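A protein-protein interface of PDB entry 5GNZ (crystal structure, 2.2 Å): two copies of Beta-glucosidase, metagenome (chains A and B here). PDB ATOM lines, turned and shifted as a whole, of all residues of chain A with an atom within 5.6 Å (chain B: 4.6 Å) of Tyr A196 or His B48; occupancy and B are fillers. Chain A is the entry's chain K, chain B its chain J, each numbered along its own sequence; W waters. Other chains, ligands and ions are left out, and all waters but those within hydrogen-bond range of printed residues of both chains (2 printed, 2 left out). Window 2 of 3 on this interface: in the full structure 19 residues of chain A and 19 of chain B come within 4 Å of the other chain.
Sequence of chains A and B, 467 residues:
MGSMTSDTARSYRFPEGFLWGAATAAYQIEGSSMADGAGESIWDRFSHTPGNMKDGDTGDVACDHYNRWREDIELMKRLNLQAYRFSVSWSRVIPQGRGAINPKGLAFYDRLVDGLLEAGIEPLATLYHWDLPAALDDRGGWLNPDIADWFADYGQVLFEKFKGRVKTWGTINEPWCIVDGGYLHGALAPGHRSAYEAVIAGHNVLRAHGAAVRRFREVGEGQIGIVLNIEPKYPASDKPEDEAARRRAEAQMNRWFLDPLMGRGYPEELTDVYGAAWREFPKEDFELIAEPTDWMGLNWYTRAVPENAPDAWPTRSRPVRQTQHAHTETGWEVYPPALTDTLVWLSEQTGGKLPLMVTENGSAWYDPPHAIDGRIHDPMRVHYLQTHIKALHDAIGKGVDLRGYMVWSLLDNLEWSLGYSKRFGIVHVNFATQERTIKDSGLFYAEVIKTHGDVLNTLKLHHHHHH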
ATOM      1  N   SER A 194      23.697  -2.488  30.186  1.00  0.00           N
ATOM      2  CA  SER A 194      22.725  -3.391  29.581  1.00  0.00           C
ATOM      3  C   SER A 194      21.784  -3.976  30.627  1.00  0.00           C
ATOM      4  O   SER A 194      22.232  -4.561  31.613  1.00  0.00           O
ATOM      5  CB  SER A 194      23.449  -4.514  28.831  1.00  0.00           C
ATOM      6  OG  SER A 194      22.526  -5.439  28.282  1.00  0.00           O
ATOM      7  N   ALA A 195      20.482  -3.819  30.412  1.00  0.00           N
ATOM      8  CA  ALA A 195      19.487  -4.392  31.313  1.00  0.00           C
ATOM      9  C   ALA A 195      19.462  -5.919  31.264  1.00  0.00           C
ATOM     10  O   ALA A 195      19.290  -6.577  32.295  1.00  0.00           O
ATOM     11  CB  ALA A 195      18.111  -3.834  30.988  1.00  0.00           C
ATOM     12  N   TYR A 196      19.630  -6.470  30.065  1.00  0.00           N
ATOM     13  CA  TYR A 196      19.680  -7.916  29.872  1.00  0.00           C
ATOM     14  C   TYR A 196      20.797  -8.508  30.742  1.00  0.00           C
ATOM     15  O   TYR A 196      20.594  -9.461  31.539  1.00  0.00           O
ATOM     16  CB  TYR A 196      19.921  -8.238  28.391  1.00  0.00           C
ATOM     17  CG  TYR A 196      18.843  -7.732  27.443  1.00  0.00           C
ATOM     18  CD1 TYR A 196      18.910  -6.452  26.899  1.00  0.00           C
ATOM     19  CD2 TYR A 196      17.772  -8.536  27.081  1.00  0.00           C
ATOM     20  CE1 TYR A 196      17.933  -5.986  26.035  1.00  0.00           C
ATOM     21  CE2 TYR A 196      16.790  -8.078  26.218  1.00  0.00           C
ATOM     22  CZ  TYR A 196      16.875  -6.805  25.700  1.00  0.00           C
ATOM     23  OH  TYR A 196      15.899  -6.350  24.840  1.00  0.00           O
ATOM     24  N   GLU A 197      21.963  -7.874  30.641  1.00  0.00           N
ATOM     25  CA  GLU A 197      23.143  -8.312  31.365  1.00  0.00           C
ATOM     26  C   GLU A 197      22.954  -8.071  32.850  1.00  0.00           C
ATOM     27  O   GLU A 197      23.427  -8.847  33.660  1.00  0.00           O
ATOM     28  CB  GLU A 197      24.399  -7.591  30.864  1.00  0.00           C
ATOM     29  CG  GLU A 197      24.832  -7.965  29.453  1.00  0.00           C
ATOM     30  CD  GLU A 197      26.139  -7.305  29.064  1.00  0.00           C
ATOM     31  OE1 GLU A 197      26.883  -6.891  29.976  1.00  0.00           O
ATOM     32  OE2 GLU A 197      26.417  -7.197  27.851  1.00  0.00           O
ATOM     33  N   ALA A 198      22.298  -6.971  33.203  1.00  0.00           N
ATOM     34  CA  ALA A 198      22.041  -6.656  34.603  1.00  0.00           C
ATOM     35  C   ALA A 198      21.206  -7.754  35.267  1.00  0.00           C
ATOM     36  O   ALA A 198      21.522  -8.211  36.372  1.00  0.00           O
ATOM     37  CB  ALA A 198      21.349  -5.309  34.721  1.00  0.00           C
ATOM     38  N   VAL A 199      20.150  -8.191  34.584  1.00  0.00           N
ATOM     39  CA  VAL A 199      19.294  -9.249  35.116  1.00  0.00           C
ATOM     40  C   VAL A 199      20.090 -10.540  35.302  1.00  0.00           C
ATOM     41  O   VAL A 199      20.095 -11.152  36.400  1.00  0.00           O
ATOM     42  CB  VAL A 199      18.093  -9.517  34.179  1.00  0.00           C
ATOM     43  CG1 VAL A 199      17.385 -10.800  34.567  1.00  0.00           C
ATOM     44  CG2 VAL A 199      17.124  -8.347  34.195  1.00  0.00           C
ATOM     45  N   ILE A 200      20.826 -10.914  34.255  1.00  0.00           N
ATOM     46  CA  ILE A 200      21.627 -12.136  34.330  1.00  0.00           C
ATOM     47  C   ILE A 200      22.693 -12.091  35.442  1.00  0.00           C
ATOM     48  O   ILE A 200      22.838 -13.039  36.229  1.00  0.00           O
ATOM     49  CB  ILE A 200      22.306 -12.415  32.974  1.00  0.00           C
ATOM     50  CG1 ILE A 200      21.251 -12.752  31.919  1.00  0.00           C
ATOM     51  CG2 ILE A 200      23.323 -13.534  33.092  1.00  0.00           C
ATOM     52  CD1 ILE A 200      21.763 -12.696  30.501  1.00  0.00           C
ATOM     53  N   ALA A 201      23.413 -10.978  35.515  1.00  0.00           N
ATOM     54  CA  ALA A 201      24.467 -10.774  36.505  1.00  0.00           C
ATOM     55  C   ALA A 201      23.937 -10.810  37.931  1.00  0.00           C
ATOM     56  O   ALA A 201      24.561 -11.409  38.809  1.00  0.00           O
ATOM     57  CB  ALA A 201      25.187  -9.455  36.246  1.00  0.00           C
ATOM     58  N   ALA A 276      11.435  -6.462  28.455  1.00  0.00           N
ATOM     59  CA  ALA A 276      11.861  -7.581  27.627  1.00  0.00           C
ATOM     60  C   ALA A 276      13.175  -8.208  28.079  1.00  0.00           C
ATOM     61  O   ALA A 276      13.512  -9.316  27.663  1.00  0.00           O
ATOM     62  CB  ALA A 276      11.972  -7.134  26.185  1.00  0.00           C
ATOM     63  N   ALA A 277      13.916  -7.502  28.927  1.00  0.00           N
ATOM     64  CA  ALA A 277      15.182  -8.022  29.424  1.00  0.00           C
ATOM     65  C   ALA A 277      14.987  -8.962  30.603  1.00  0.00           C
ATOM     66  O   ALA A 277      15.892  -9.715  30.954  1.00  0.00           O
ATOM     67  CB  ALA A 277      16.100  -6.879  29.818  1.00  0.00           C
ATOM     68  N   ARG A 279      13.836 -12.152  32.795  1.00  0.00           N
ATOM     69  CA  ARG A 279      13.888 -13.571  32.486  1.00  0.00           C
ATOM     70  C   ARG A 279      13.280 -14.412  33.592  1.00  0.00           C
ATOM     71  O   ARG A 279      13.264 -14.008  34.756  1.00  0.00           O
ATOM     72  CB  ARG A 279      15.336 -14.009  32.266  1.00  0.00           C
ATOM     73  CG  ARG A 279      16.007 -13.412  31.055  1.00  0.00           C
ATOM     74  CD  ARG A 279      15.543 -14.101  29.788  1.00  0.00           C
ATOM     75  NE  ARG A 279      16.247 -13.589  28.619  1.00  0.00           N
ATOM     76  CZ  ARG A 279      15.833 -12.556  27.894  1.00  0.00           C
ATOM     77  NH1 ARG A 279      14.715 -11.919  28.215  1.00  0.00           N
ATOM     78  NH2 ARG A 279      16.539 -12.160  26.846  1.00  0.00           N
ATOM     79  N   TRP A 313      16.010   5.696  32.740  1.00  0.00           N
ATOM     80  CA  TRP A 313      16.080   4.271  32.446  1.00  0.00           C
ATOM     81  C   TRP A 313      16.867   3.524  33.518  1.00  0.00           C
ATOM     82  O   TRP A 313      17.937   3.969  33.922  1.00  0.00           O
ATOM     83  CB  TRP A 313      16.700   4.065  31.064  1.00  0.00           C
ATOM     84  CG  TRP A 313      16.913   2.643  30.662  1.00  0.00           C
ATOM     85  CD1 TRP A 313      16.005   1.801  30.084  1.00  0.00           C
ATOM     86  CD2 TRP A 313      18.136   1.907  30.761  1.00  0.00           C
ATOM     87  NE1 TRP A 313      16.586   0.581  29.840  1.00  0.00           N
ATOM     88  CE2 TRP A 313      17.895   0.620  30.246  1.00  0.00           C
ATOM     89  CE3 TRP A 313      19.411   2.211  31.245  1.00  0.00           C
ATOM     90  CZ2 TRP A 313      18.884  -0.364  30.200  1.00  0.00           C
ATOM     91  CZ3 TRP A 313      20.388   1.235  31.201  1.00  0.00           C
ATOM     92  CH2 TRP A 313      20.121  -0.036  30.682  1.00  0.00           C
ATOM     93  N   GLU B  40      18.891 -15.218  20.767  1.00  0.00           N
ATOM     94  CA  GLU B  40      19.194 -13.815  21.009  1.00  0.00           C
ATOM     95  C   GLU B  40      20.652 -13.517  20.660  1.00  0.00           C
ATOM     96  O   GLU B  40      21.550 -14.236  21.093  1.00  0.00           O
ATOM     97  CB  GLU B  40      18.897 -13.476  22.474  1.00  0.00           C
ATOM     98  CG  GLU B  40      19.222 -12.056  22.903  1.00  0.00           C
ATOM     99  CD  GLU B  40      18.755 -11.777  24.319  1.00  0.00           C
ATOM    100  OE1 GLU B  40      17.604 -11.326  24.491  1.00  0.00           O
ATOM    101  OE2 GLU B  40      19.533 -12.025  25.261  1.00  0.00           O
ATOM    102  N   ASP B  44      20.554  -7.890  19.337  1.00  0.00           N
ATOM    103  CA  ASP B  44      19.217  -7.887  19.923  1.00  0.00           C
ATOM    104  C   ASP B  44      19.235  -7.097  21.228  1.00  0.00           C
ATOM    105  O   ASP B  44      18.373  -6.252  21.473  1.00  0.00           O
ATOM    106  CB  ASP B  44      18.720  -9.315  20.173  1.00  0.00           C
ATOM    107  CG  ASP B  44      18.399 -10.057  18.890  1.00  0.00           C
ATOM    108  OD1 ASP B  44      17.749  -9.460  18.009  1.00  0.00           O
ATOM    109  OD2 ASP B  44      18.785 -11.239  18.770  1.00  0.00           O
ATOM    110  N   ARG B  45      20.229  -7.388  22.060  1.00  0.00           N
ATOM    111  CA  ARG B  45      20.426  -6.692  23.328  1.00  0.00           C
ATOM    112  C   ARG B  45      20.833  -5.234  23.129  1.00  0.00           C
ATOM    113  O   ARG B  45      20.243  -4.330  23.716  1.00  0.00           O
ATOM    114  CB  ARG B  45      21.492  -7.404  24.160  1.00  0.00           C
ATOM    115  CG  ARG B  45      21.112  -8.787  24.642  1.00  0.00           C
ATOM    116  CD  ARG B  45      22.233  -9.379  25.483  1.00  0.00           C
ATOM    117  NE  ARG B  45      21.860 -10.657  26.077  1.00  0.00           N
ATOM    118  CZ  ARG B  45      22.679 -11.407  26.805  1.00  0.00           C
ATOM    119  NH1 ARG B  45      23.923 -11.011  27.028  1.00  0.00           N
ATOM    120  NH2 ARG B  45      22.255 -12.558  27.301  1.00  0.00           N
ATOM    121  N   PHE B  46      21.855  -5.026  22.303  1.00  0.00           N
ATOM    122  CA  PHE B  46      22.443  -3.707  22.088  1.00  0.00           C
ATOM    123  C   PHE B  46      21.437  -2.702  21.538  1.00  0.00           C
ATOM    124  O   PHE B  46      21.345  -1.576  22.027  1.00  0.00           O
ATOM    125  CB  PHE B  46      23.640  -3.817  21.139  1.00  0.00           C
ATOM    126  CG  PHE B  46      24.498  -2.586  21.092  1.00  0.00           C
ATOM    127  CD1 PHE B  46      25.473  -2.377  22.053  1.00  0.00           C
ATOM    128  CD2 PHE B  46      24.340  -1.646  20.082  1.00  0.00           C
ATOM    129  CE1 PHE B  46      26.270  -1.250  22.017  1.00  0.00           C
ATOM    130  CE2 PHE B  46      25.136  -0.518  20.039  1.00  0.00           C
ATOM    131  CZ  PHE B  46      26.103  -0.318  21.007  1.00  0.00           C
ATOM    132  N   SER B  47      20.677  -3.115  20.529  1.00  0.00           N
ATOM    133  CA  SER B  47      19.751  -2.206  19.864  1.00  0.00           C
ATOM    134  C   SER B  47      18.548  -1.858  20.734  1.00  0.00           C
ATOM    135  O   SER B  47      17.871  -0.855  20.493  1.00  0.00           O
ATOM    136  CB  SER B  47      19.276  -2.809  18.542  1.00  0.00           C
ATOM    137  OG  SER B  47      18.392  -3.891  18.763  1.00  0.00           O
ATOM    138  N   HIS B  48      18.279  -2.682  21.742  1.00  0.00           N
ATOM    139  CA  HIS B  48      17.160  -2.437  22.645  1.00  0.00           C
ATOM    140  C   HIS B  48      17.633  -1.837  23.963  1.00  0.00           C
ATOM    141  O   HIS B  48      16.955  -1.936  24.984  1.00  0.00           O
ATOM    142  CB  HIS B  48      16.376  -3.725  22.896  1.00  0.00           C
ATOM    143  CG  HIS B  48      15.469  -4.111  21.767  1.00  0.00           C
ATOM    144  ND1 HIS B  48      15.866  -4.944  20.742  1.00  0.00           N
ATOM    145  CD2 HIS B  48      14.188  -3.766  21.497  1.00  0.00           C
ATOM    146  CE1 HIS B  48      14.861  -5.104  19.896  1.00  0.00           C
ATOM    147  NE2 HIS B  48      13.834  -4.396  20.329  1.00  0.00           N
ATOM    148  N   THR B  49      18.807  -1.219  23.930  1.00  0.00           N
ATOM    149  CA  THR B  49      19.304  -0.471  25.069  1.00  0.00           C
ATOM    150  C   THR B  49      19.282   0.988  24.658  1.00  0.00           C
ATOM    151  O   THR B  49      19.923   1.365  23.678  1.00  0.00           O
ATOM    152  CB  THR B  49      20.727  -0.900  25.467  1.00  0.00           C
ATOM    153  OG1 THR B  49      20.760  -2.315  25.697  1.00  0.00           O
ATOM    154  CG2 THR B  49      21.181  -0.175  26.721  1.00  0.00           C
ATOM    155  N   PRO B  50      18.536   1.815  25.404  1.00  0.00           N
ATOM    156  CA  PRO B  50      18.328   3.216  25.014  1.00  0.00           C
ATOM    157  C   PRO B  50      19.624   4.014  24.932  1.00  0.00           C
ATOM    158  O   PRO B  50      20.499   3.870  25.784  1.00  0.00           O
ATOM    159  CB  PRO B  50      17.414   3.764  26.124  1.00  0.00           C
ATOM    160  CG  PRO B  50      17.550   2.805  27.262  1.00  0.00           C
ATOM    161  CD  PRO B  50      17.822   1.470  26.646  1.00  0.00           C
ATOM    162  N   THR B  58      15.974  -0.413  15.522  1.00  0.00           N
ATOM    163  CA  THR B  58      16.427  -1.781  15.768  1.00  0.00           C
ATOM    164  C   THR B  58      16.323  -2.607  14.490  1.00  0.00           C
ATOM    165  O   THR B  58      15.734  -2.165  13.501  1.00  0.00           O
ATOM    166  CB  THR B  58      15.612  -2.480  16.888  1.00  0.00           C
ATOM    167  OG1 THR B  58      14.351  -2.910  16.365  1.00  0.00           O
ATOM    168  CG2 THR B  58      15.375  -1.547  18.073  1.00  0.00           C
ATOM    169  N   ASP B  60      14.634  -5.373  14.347  1.00  0.00           N
ATOM    170  CA  ASP B  60      13.470  -6.239  14.553  1.00  0.00           C
ATOM    171  C   ASP B  60      12.747  -6.556  13.248  1.00  0.00           C
ATOM    172  O   ASP B  60      12.329  -7.690  13.017  1.00  0.00           O
ATOM    173  CB  ASP B  60      12.479  -5.591  15.525  1.00  0.00           C
ATOM    174  CG  ASP B  60      12.930  -5.672  16.968  1.00  0.00           C
ATOM    175  OD1 ASP B  60      13.947  -6.339  17.245  1.00  0.00           O
ATOM    176  OD2 ASP B  60      12.249  -5.076  17.830  1.00  0.00           O
HETATM  177  O   HOH W   1      22.018  -4.685  25.953  1.00  0.00           O
HETATM  178  O   HOH W   2      19.308  -2.974  28.028  1.00  0.00           O
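Of the printed residues of chain B, Tyr A196 touches Glu B40, Arg B45 and His B48. His B48 touches just one residue of chain A: Tyr A196. Of the printed residues of chain A, Arg B45 touches Tyr A196, Glu A197 and Ile A200. Of the printed residues of chain A, Glu B40 touches Tyr A196 (3.8 Å) and Arg A279 (2.7 Å). Of the printed residues of chain B, Arg A279 touches Glu B40. Asp B60 touches none of the printed residues of chain A. Val A199 touches none of the printed residues of chain B. The nearest residue of chain A that does not touch His B48 is Trp A313 (5.5 Å). The nearest printed residue of chain B that does not touch Ile A200 is Glu B40 (5.7 Å).
A ring nitrogen (ND1) of His B48 lies within hydrogen-bond range of the backbone carbonyl oxygen (O) of Asp B44 (2.9 Å). O of Arg B45 is in hydrogen-bond range of OG1 of Thr B49 (2.9 Å). The side-chain hydroxyl (OG) of Ser B47 lies within hydrogen-bond range of a ring nitrogen (ND1) of His B48 (3.4 Å). OD2 of Asp B60 lies within hydrogen-bond range of NE2 of His B48 (3.0 Å). N of Glu A197 sits at hydrogen-bond distance from OG of Ser A194 (3.4 Å). The guanidinium group (NH1) of Arg A279 sits at hydrogen-bond distance from the backbone carbonyl oxygen (O) of Ala A276 (2.9 Å).
Water W1 lies within hydrogen-bond range of OG of Ser A194 (2.5 Å), OG1 of Thr B49 (2.7 Å) and O of Arg B45 (2.9 Å). Water W2 bridges the backbone NH of Ala A195 (2.8 Å) and the side-chain hydroxyl of Thr B49 (2.8 Å).
Tyr A196 touches Glu B40 (CE2 to OE1, 3.8 Å). Tyr A196 touches Arg B45. His B48 touches Tyr A196 (CB to OH, 3.3 Å). Glu A197 touches Arg B45. Arg B45 touches Ile A200. Pro B50 touches Trp A313 (CG to CD1, 3.4 Å).
No position is printed for both chains. Of the 7 pairs that touch across the chains among the printed residues, none has its exchanged pair printed and touching as well.
Hydrophobic or aromatic side chains of chain A within 4 Å of the printed part of chain B: Tyr A196, Ile A200 and Trp A313. Of the 10 printed residues of chain B, 4 touch a printed residue of chain A. Hydrophobic or aromatic side chains of chain B within 4 Å of the printed part of chain A: His B48 and Pro B50.
OE1 of Glu B40 lies within salt-bridge range of NH2 of Arg A279 (2.7 Å).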
